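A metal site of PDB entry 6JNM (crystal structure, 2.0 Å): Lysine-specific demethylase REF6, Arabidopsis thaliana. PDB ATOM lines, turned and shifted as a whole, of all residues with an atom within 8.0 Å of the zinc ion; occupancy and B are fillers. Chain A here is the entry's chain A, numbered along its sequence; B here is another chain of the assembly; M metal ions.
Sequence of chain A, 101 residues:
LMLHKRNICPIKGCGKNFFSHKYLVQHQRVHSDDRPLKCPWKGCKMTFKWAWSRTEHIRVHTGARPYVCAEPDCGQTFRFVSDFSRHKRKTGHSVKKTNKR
The zinc ion is bound by a ring nitrogen (NE2) of His 61, a ring nitrogen (NE2) of His 57, the side-chain sulfur (SG) of Cys 44 and the side-chain sulfur (SG) of Cys 39.
Within 4 Å of the zinc ion: Cys 39, Cys 44, His 57 and His 61. The nearest printed residue that does not touch the zinc ion is Trp 41 (4.2 Å).
The side-chain sulfur (SG) of Cys 44 lies close to the backbone NH (N) of Met 46 (3.5 Å). The backbone NH (N) of Trp 41 sits close to the side-chain sulfur (SG) of Cys 39 (3.4 Å). ND1 of His 57 is in hydrogen-bond range of OP1 of DT 4 of chain B (2.7 Å). The backbone NH of Cys 39 lies within hydrogen-bond range of the backbone carbonyl oxygen of Met 46, at 3.2 Å.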
ATOM      1  N   LYS A  38      10.474   6.252  27.976  1.00  0.00           N
ATOM      2  CA  LYS A  38      11.145   5.383  27.029  1.00  0.00           C
ATOM      3  C   LYS A  38      10.343   5.423  25.768  1.00  0.00           C
ATOM      4  O   LYS A  38       9.142   5.607  25.819  1.00  0.00           O
ATOM      5  CB  LYS A  38      11.138   3.957  27.551  1.00  0.00           C
ATOM      6  CG  LYS A  38      12.264   3.675  28.520  1.00  0.00           C
ATOM      7  CD  LYS A  38      13.401   2.887  27.815  1.00  0.00           C
ATOM      8  CE  LYS A  38      14.817   3.155  28.333  1.00  0.00           C
ATOM      9  NZ  LYS A  38      14.981   2.627  29.703  1.00  0.00           N
ATOM     10  N   CYS A  39      11.011   5.230  24.646  1.00  0.00           N
ATOM     11  CA  CYS A  39      10.324   5.132  23.372  1.00  0.00           C
ATOM     12  C   CYS A  39       9.741   3.747  23.335  1.00  0.00           C
ATOM     13  O   CYS A  39      10.483   2.809  23.628  1.00  0.00           O
ATOM     14  CB  CYS A  39      11.308   5.210  22.209  1.00  0.00           C
ATOM     15  SG  CYS A  39      10.503   5.077  20.575  1.00  0.00           S
ATOM     16  N   PRO A  40       8.484   3.583  22.866  1.00  0.00           N
ATOM     17  CA  PRO A  40       7.986   2.226  22.815  1.00  0.00           C
ATOM     18  C   PRO A  40       8.379   1.445  21.544  1.00  0.00           C
ATOM     19  O   PRO A  40       7.958   0.349  21.398  1.00  0.00           O
ATOM     20  CB  PRO A  40       6.482   2.445  22.844  1.00  0.00           C
ATOM     21  CG  PRO A  40       6.355   3.708  21.992  1.00  0.00           C
ATOM     22  CD  PRO A  40       7.436   4.552  22.530  1.00  0.00           C
ATOM     23  N   TRP A  41       9.154   1.963  20.639  1.00  0.00           N
ATOM     24  CA  TRP A  41       9.374   1.299  19.384  1.00  0.00           C
ATOM     25  C   TRP A  41      10.475   0.335  19.629  1.00  0.00           C
ATOM     26  O   TRP A  41      11.498   0.675  20.233  1.00  0.00           O
ATOM     27  CB  TRP A  41       9.913   2.271  18.325  1.00  0.00           C
ATOM     28  CG  TRP A  41       9.800   1.804  16.919  1.00  0.00           C
ATOM     29  CD1 TRP A  41      10.798   1.229  16.105  1.00  0.00           C
ATOM     30  CD2 TRP A  41       8.629   1.906  16.105  1.00  0.00           C
ATOM     31  NE1 TRP A  41      10.274   1.017  14.839  1.00  0.00           N
ATOM     32  CE2 TRP A  41       8.976   1.429  14.821  1.00  0.00           C
ATOM     33  CE3 TRP A  41       7.348   2.396  16.326  1.00  0.00           C
ATOM     34  CZ2 TRP A  41       8.077   1.391  13.803  1.00  0.00           C
ATOM     35  CZ3 TRP A  41       6.474   2.398  15.327  1.00  0.00           C
ATOM     36  CH2 TRP A  41       6.823   1.870  14.071  1.00  0.00           C
ATOM     37  N   LYS A  42      10.301  -0.850  19.099  1.00  0.00           N
ATOM     38  CA  LYS A  42      11.215  -1.923  19.435  1.00  0.00           C
ATOM     39  C   LYS A  42      12.599  -1.647  18.933  1.00  0.00           C
ATOM     40  O   LYS A  42      12.759  -1.426  17.725  1.00  0.00           O
ATOM     41  CB  LYS A  42      10.682  -3.212  18.789  1.00  0.00           C
ATOM     42  CG  LYS A  42      11.667  -4.343  18.658  1.00  0.00           C
ATOM     43  CD  LYS A  42      11.790  -5.083  19.942  1.00  0.00           C
ATOM     44  CE  LYS A  42      12.231  -6.531  19.609  1.00  0.00           C
ATOM     45  NZ  LYS A  42      12.466  -7.205  20.906  1.00  0.00           N
ATOM     46  N   GLY A  43      13.580  -1.795  19.803  1.00  0.00           N
ATOM     47  CA  GLY A  43      14.962  -1.469  19.483  1.00  0.00           C
ATOM     48  C   GLY A  43      15.408  -0.029  19.690  1.00  0.00           C
ATOM     49  O   GLY A  43      16.581   0.239  19.666  1.00  0.00           O
ATOM     50  N   CYS A  44      14.514   0.922  19.905  1.00  0.00           N
ATOM     51  CA  CYS A  44      14.930   2.308  19.892  1.00  0.00           C
ATOM     52  C   CYS A  44      15.397   2.618  21.298  1.00  0.00           C
ATOM     53  O   CYS A  44      14.714   2.339  22.226  1.00  0.00           O
ATOM     54  CB  CYS A  44      13.787   3.233  19.441  1.00  0.00           C
ATOM     55  SG  CYS A  44      14.130   4.980  19.666  1.00  0.00           S
ATOM     56  N   LYS A  45      16.526   3.282  21.444  1.00  0.00           N
ATOM     57  CA  LYS A  45      17.035   3.609  22.776  1.00  0.00           C
ATOM     58  C   LYS A  45      16.695   4.971  23.270  1.00  0.00           C
ATOM     59  O   LYS A  45      17.109   5.320  24.380  1.00  0.00           O
ATOM     60  CB  LYS A  45      18.593   3.525  22.818  1.00  0.00           C
ATOM     61  CG  LYS A  45      19.204   2.234  22.296  1.00  0.00           C
ATOM     62  CD  LYS A  45      18.932   1.088  23.258  1.00  0.00           C
ATOM     63  CE  LYS A  45      18.235  -0.083  22.595  1.00  0.00           C
ATOM     64  NZ  LYS A  45      18.287  -1.228  23.544  1.00  0.00           N
ATOM     65  N   MET A  46      15.977   5.754  22.490  1.00  0.00           N
ATOM     66  CA  MET A  46      15.688   7.135  22.909  1.00  0.00           C
ATOM     67  C   MET A  46      14.904   7.142  24.204  1.00  0.00           C
ATOM     68  O   MET A  46      14.013   6.311  24.450  1.00  0.00           O
ATOM     69  CB  MET A  46      14.874   7.826  21.791  1.00  0.00           C
ATOM     70  CG  MET A  46      14.683   9.337  21.971  1.00  0.00           C
ATOM     71  SD  MET A  46      16.242  10.222  21.774  1.00  0.00           S
ATOM     72  CE  MET A  46      17.117   9.201  20.525  1.00  0.00           C
ATOM     73  N   THR A  47      15.218   8.095  25.048  1.00  0.00           N
ATOM     74  CA  THR A  47      14.494   8.324  26.303  1.00  0.00           C
ATOM     75  C   THR A  47      14.201   9.787  26.379  1.00  0.00           C
ATOM     76  O   THR A  47      14.845  10.573  25.673  1.00  0.00           O
ATOM     77  CB  THR A  47      15.357   7.924  27.528  1.00  0.00           C
ATOM     78  OG1 THR A  47      16.485   8.754  27.542  1.00  0.00           O
ATOM     79  CG2 THR A  47      15.853   6.444  27.398  1.00  0.00           C
ATOM     80  N   PHE A  48      13.304  10.166  27.261  1.00  0.00           N
ATOM     81  CA  PHE A  48      12.802  11.497  27.360  1.00  0.00           C
ATOM     82  C   PHE A  48      12.583  11.902  28.804  1.00  0.00           C
ATOM     83  O   PHE A  48      12.428  11.060  29.731  1.00  0.00           O
ATOM     84  CB  PHE A  48      11.435  11.575  26.702  1.00  0.00           C
ATOM     85  CG  PHE A  48      11.413  10.910  25.364  1.00  0.00           C
ATOM     86  CD1 PHE A  48      11.151   9.526  25.272  1.00  0.00           C
ATOM     87  CD2 PHE A  48      11.755  11.626  24.218  1.00  0.00           C
ATOM     88  CE1 PHE A  48      11.210   8.918  24.034  1.00  0.00           C
ATOM     89  CE2 PHE A  48      11.837  11.002  22.972  1.00  0.00           C
ATOM     90  CZ  PHE A  48      11.535   9.672  22.891  1.00  0.00           C
ATOM     91  N   ARG A  54       8.199  12.537  23.764  1.00  0.00           N
ATOM     92  CA  ARG A  54       7.979  11.154  23.342  1.00  0.00           C
ATOM     93  C   ARG A  54       6.875  11.036  22.277  1.00  0.00           C
ATOM     94  O   ARG A  54       7.025  10.285  21.311  1.00  0.00           O
ATOM     95  CB  ARG A  54       7.682  10.269  24.549  1.00  0.00           C
ATOM     96  CG  ARG A  54       7.285   8.831  24.324  1.00  0.00           C
ATOM     97  CD  ARG A  54       7.048   8.158  25.698  1.00  0.00           C
ATOM     98  NE  ARG A  54       6.590   6.800  25.525  1.00  0.00           N
ATOM     99  CZ  ARG A  54       5.318   6.459  25.218  1.00  0.00           C
ATOM    100  NH1 ARG A  54       4.340   7.373  25.098  1.00  0.00           N
ATOM    101  NH2 ARG A  54       5.016   5.194  25.029  1.00  0.00           N
ATOM    102  N   HIS A  57       8.209  12.260  18.968  1.00  0.00           N
ATOM    103  CA  HIS A  57       9.236  11.372  18.543  1.00  0.00           C
ATOM    104  C   HIS A  57       8.719  10.095  17.867  1.00  0.00           C
ATOM    105  O   HIS A  57       9.336   9.535  16.921  1.00  0.00           O
ATOM    106  CB  HIS A  57      10.167  11.021  19.709  1.00  0.00           C
ATOM    107  CG  HIS A  57      11.058   9.871  19.418  1.00  0.00           C
ATOM    108  ND1 HIS A  57      12.247  10.000  18.712  1.00  0.00           N
ATOM    109  CD2 HIS A  57      10.883   8.554  19.637  1.00  0.00           C
ATOM    110  CE1 HIS A  57      12.795   8.802  18.582  1.00  0.00           C
ATOM    111  NE2 HIS A  57      12.016   7.921  19.186  1.00  0.00           N
ATOM    112  N   ILE A  58       7.633   9.591  18.400  1.00  0.00           N
ATOM    113  CA  ILE A  58       7.079   8.362  17.858  1.00  0.00           C
ATOM    114  C   ILE A  58       6.714   8.539  16.396  1.00  0.00           C
ATOM    115  O   ILE A  58       6.823   7.594  15.632  1.00  0.00           O
ATOM    116  CB  ILE A  58       5.885   7.853  18.666  1.00  0.00           C
ATOM    117  CG1 ILE A  58       6.409   7.307  20.033  1.00  0.00           C
ATOM    118  CG2 ILE A  58       5.197   6.671  17.978  1.00  0.00           C
ATOM    119  CD1 ILE A  58       5.302   7.290  21.073  1.00  0.00           C
ATOM    120  N   ARG A  59       6.380   9.753  15.988  1.00  0.00           N
ATOM    121  CA  ARG A  59       6.075  10.019  14.575  1.00  0.00           C
ATOM    122  C   ARG A  59       7.228   9.832  13.639  1.00  0.00           C
ATOM    123  O   ARG A  59       7.012   9.542  12.466  1.00  0.00           O
ATOM    124  CB  ARG A  59       5.447  11.402  14.403  1.00  0.00           C
ATOM    125  CG  ARG A  59       4.254  11.577  15.320  1.00  0.00           C
ATOM    126  CD  ARG A  59       3.589  12.897  15.061  1.00  0.00           C
ATOM    127  NE  ARG A  59       2.806  13.438  16.162  1.00  0.00           N
ATOM    128  CZ  ARG A  59       3.045  14.613  16.722  1.00  0.00           C
ATOM    129  NH1 ARG A  59       4.041  15.410  16.326  1.00  0.00           N
ATOM    130  NH2 ARG A  59       2.289  15.008  17.725  1.00  0.00           N
ATOM    131  N   VAL A  60       8.442   9.966  14.148  1.00  0.00           N
ATOM    132  CA  VAL A  60       9.641   9.654  13.369  1.00  0.00           C
ATOM    133  C   VAL A  60       9.651   8.187  12.954  1.00  0.00           C
ATOM    134  O   VAL A  60      10.025   7.894  11.876  1.00  0.00           O
ATOM    135  CB  VAL A  60      10.916   9.885  14.179  1.00  0.00           C
ATOM    136  CG1 VAL A  60      12.142   9.474  13.390  1.00  0.00           C
ATOM    137  CG2 VAL A  60      11.070  11.362  14.501  1.00  0.00           C
ATOM    138  N   HIS A  61       9.246   7.282  13.824  1.00  0.00           N
ATOM    139  CA  HIS A  61       9.101   5.850  13.461  1.00  0.00           C
ATOM    140  C   HIS A  61       7.910   5.611  12.543  1.00  0.00           C
ATOM    141  O   HIS A  61       8.052   4.907  11.591  1.00  0.00           O
ATOM    142  CB  HIS A  61       9.005   4.930  14.672  1.00  0.00           C
ATOM    143  CG  HIS A  61      10.178   4.999  15.619  1.00  0.00           C
ATOM    144  ND1 HIS A  61      11.413   4.530  15.273  1.00  0.00           N
ATOM    145  CD2 HIS A  61      10.299   5.467  16.887  1.00  0.00           C
ATOM    146  CE1 HIS A  61      12.263   4.716  16.266  1.00  0.00           C
ATOM    147  NE2 HIS A  61      11.621   5.283  17.281  1.00  0.00           N
ATOM    148  P    DT B   4      12.866  13.520  17.785  1.00  0.00           P
ATOM    149  OP1  DT B   4      13.484  12.316  18.093  1.00  0.00           O
ATOM    150  OP2  DT B   4      11.472  13.592  17.726  1.00  0.00           O
ATOM    151  O5'  DT B   4      13.351  14.627  18.795  1.00  0.00           O
ATOM    152  C5'  DT B   4      14.710  14.711  19.227  1.00  0.00           C
ATOM    153  C4'  DT B   4      14.902  15.805  20.243  1.00  0.00           C
ATOM    154  O4'  DT B   4      14.477  17.052  19.678  1.00  0.00           O
ATOM    155  C3'  DT B   4      14.139  15.649  21.563  1.00  0.00           C
ATOM    156  O3'  DT B   4      15.048  15.784  22.648  1.00  0.00           O
ATOM    157  C2'  DT B   4      13.027  16.690  21.445  1.00  0.00           C
ATOM    158  C1'  DT B   4      13.637  17.740  20.545  1.00  0.00           C
ATOM    159  N1   DT B   4      12.700  18.540  19.737  1.00  0.00           N
ATOM    160  C2   DT B   4      12.798  19.903  19.783  1.00  0.00           C
ATOM    161  O2   DT B   4      13.630  20.484  20.439  1.00  0.00           O
ATOM    162  N3   DT B   4      11.877  20.576  19.021  1.00  0.00           N
ATOM    163  C4   DT B   4      10.905  20.027  18.225  1.00  0.00           C
ATOM    164  O4   DT B   4      10.159  20.758  17.602  1.00  0.00           O
ATOM    165  C5   DT B   4      10.853  18.587  18.214  1.00  0.00           C
ATOM    166  C7   DT B   4       9.810  17.908  17.392  1.00  0.00           C
ATOM    167  C6   DT B   4      11.749  17.928  18.952  1.00  0.00           C
HETATM  168 ZN    ZN M   1      12.119   5.779  19.165  1.00  0.00          ZN
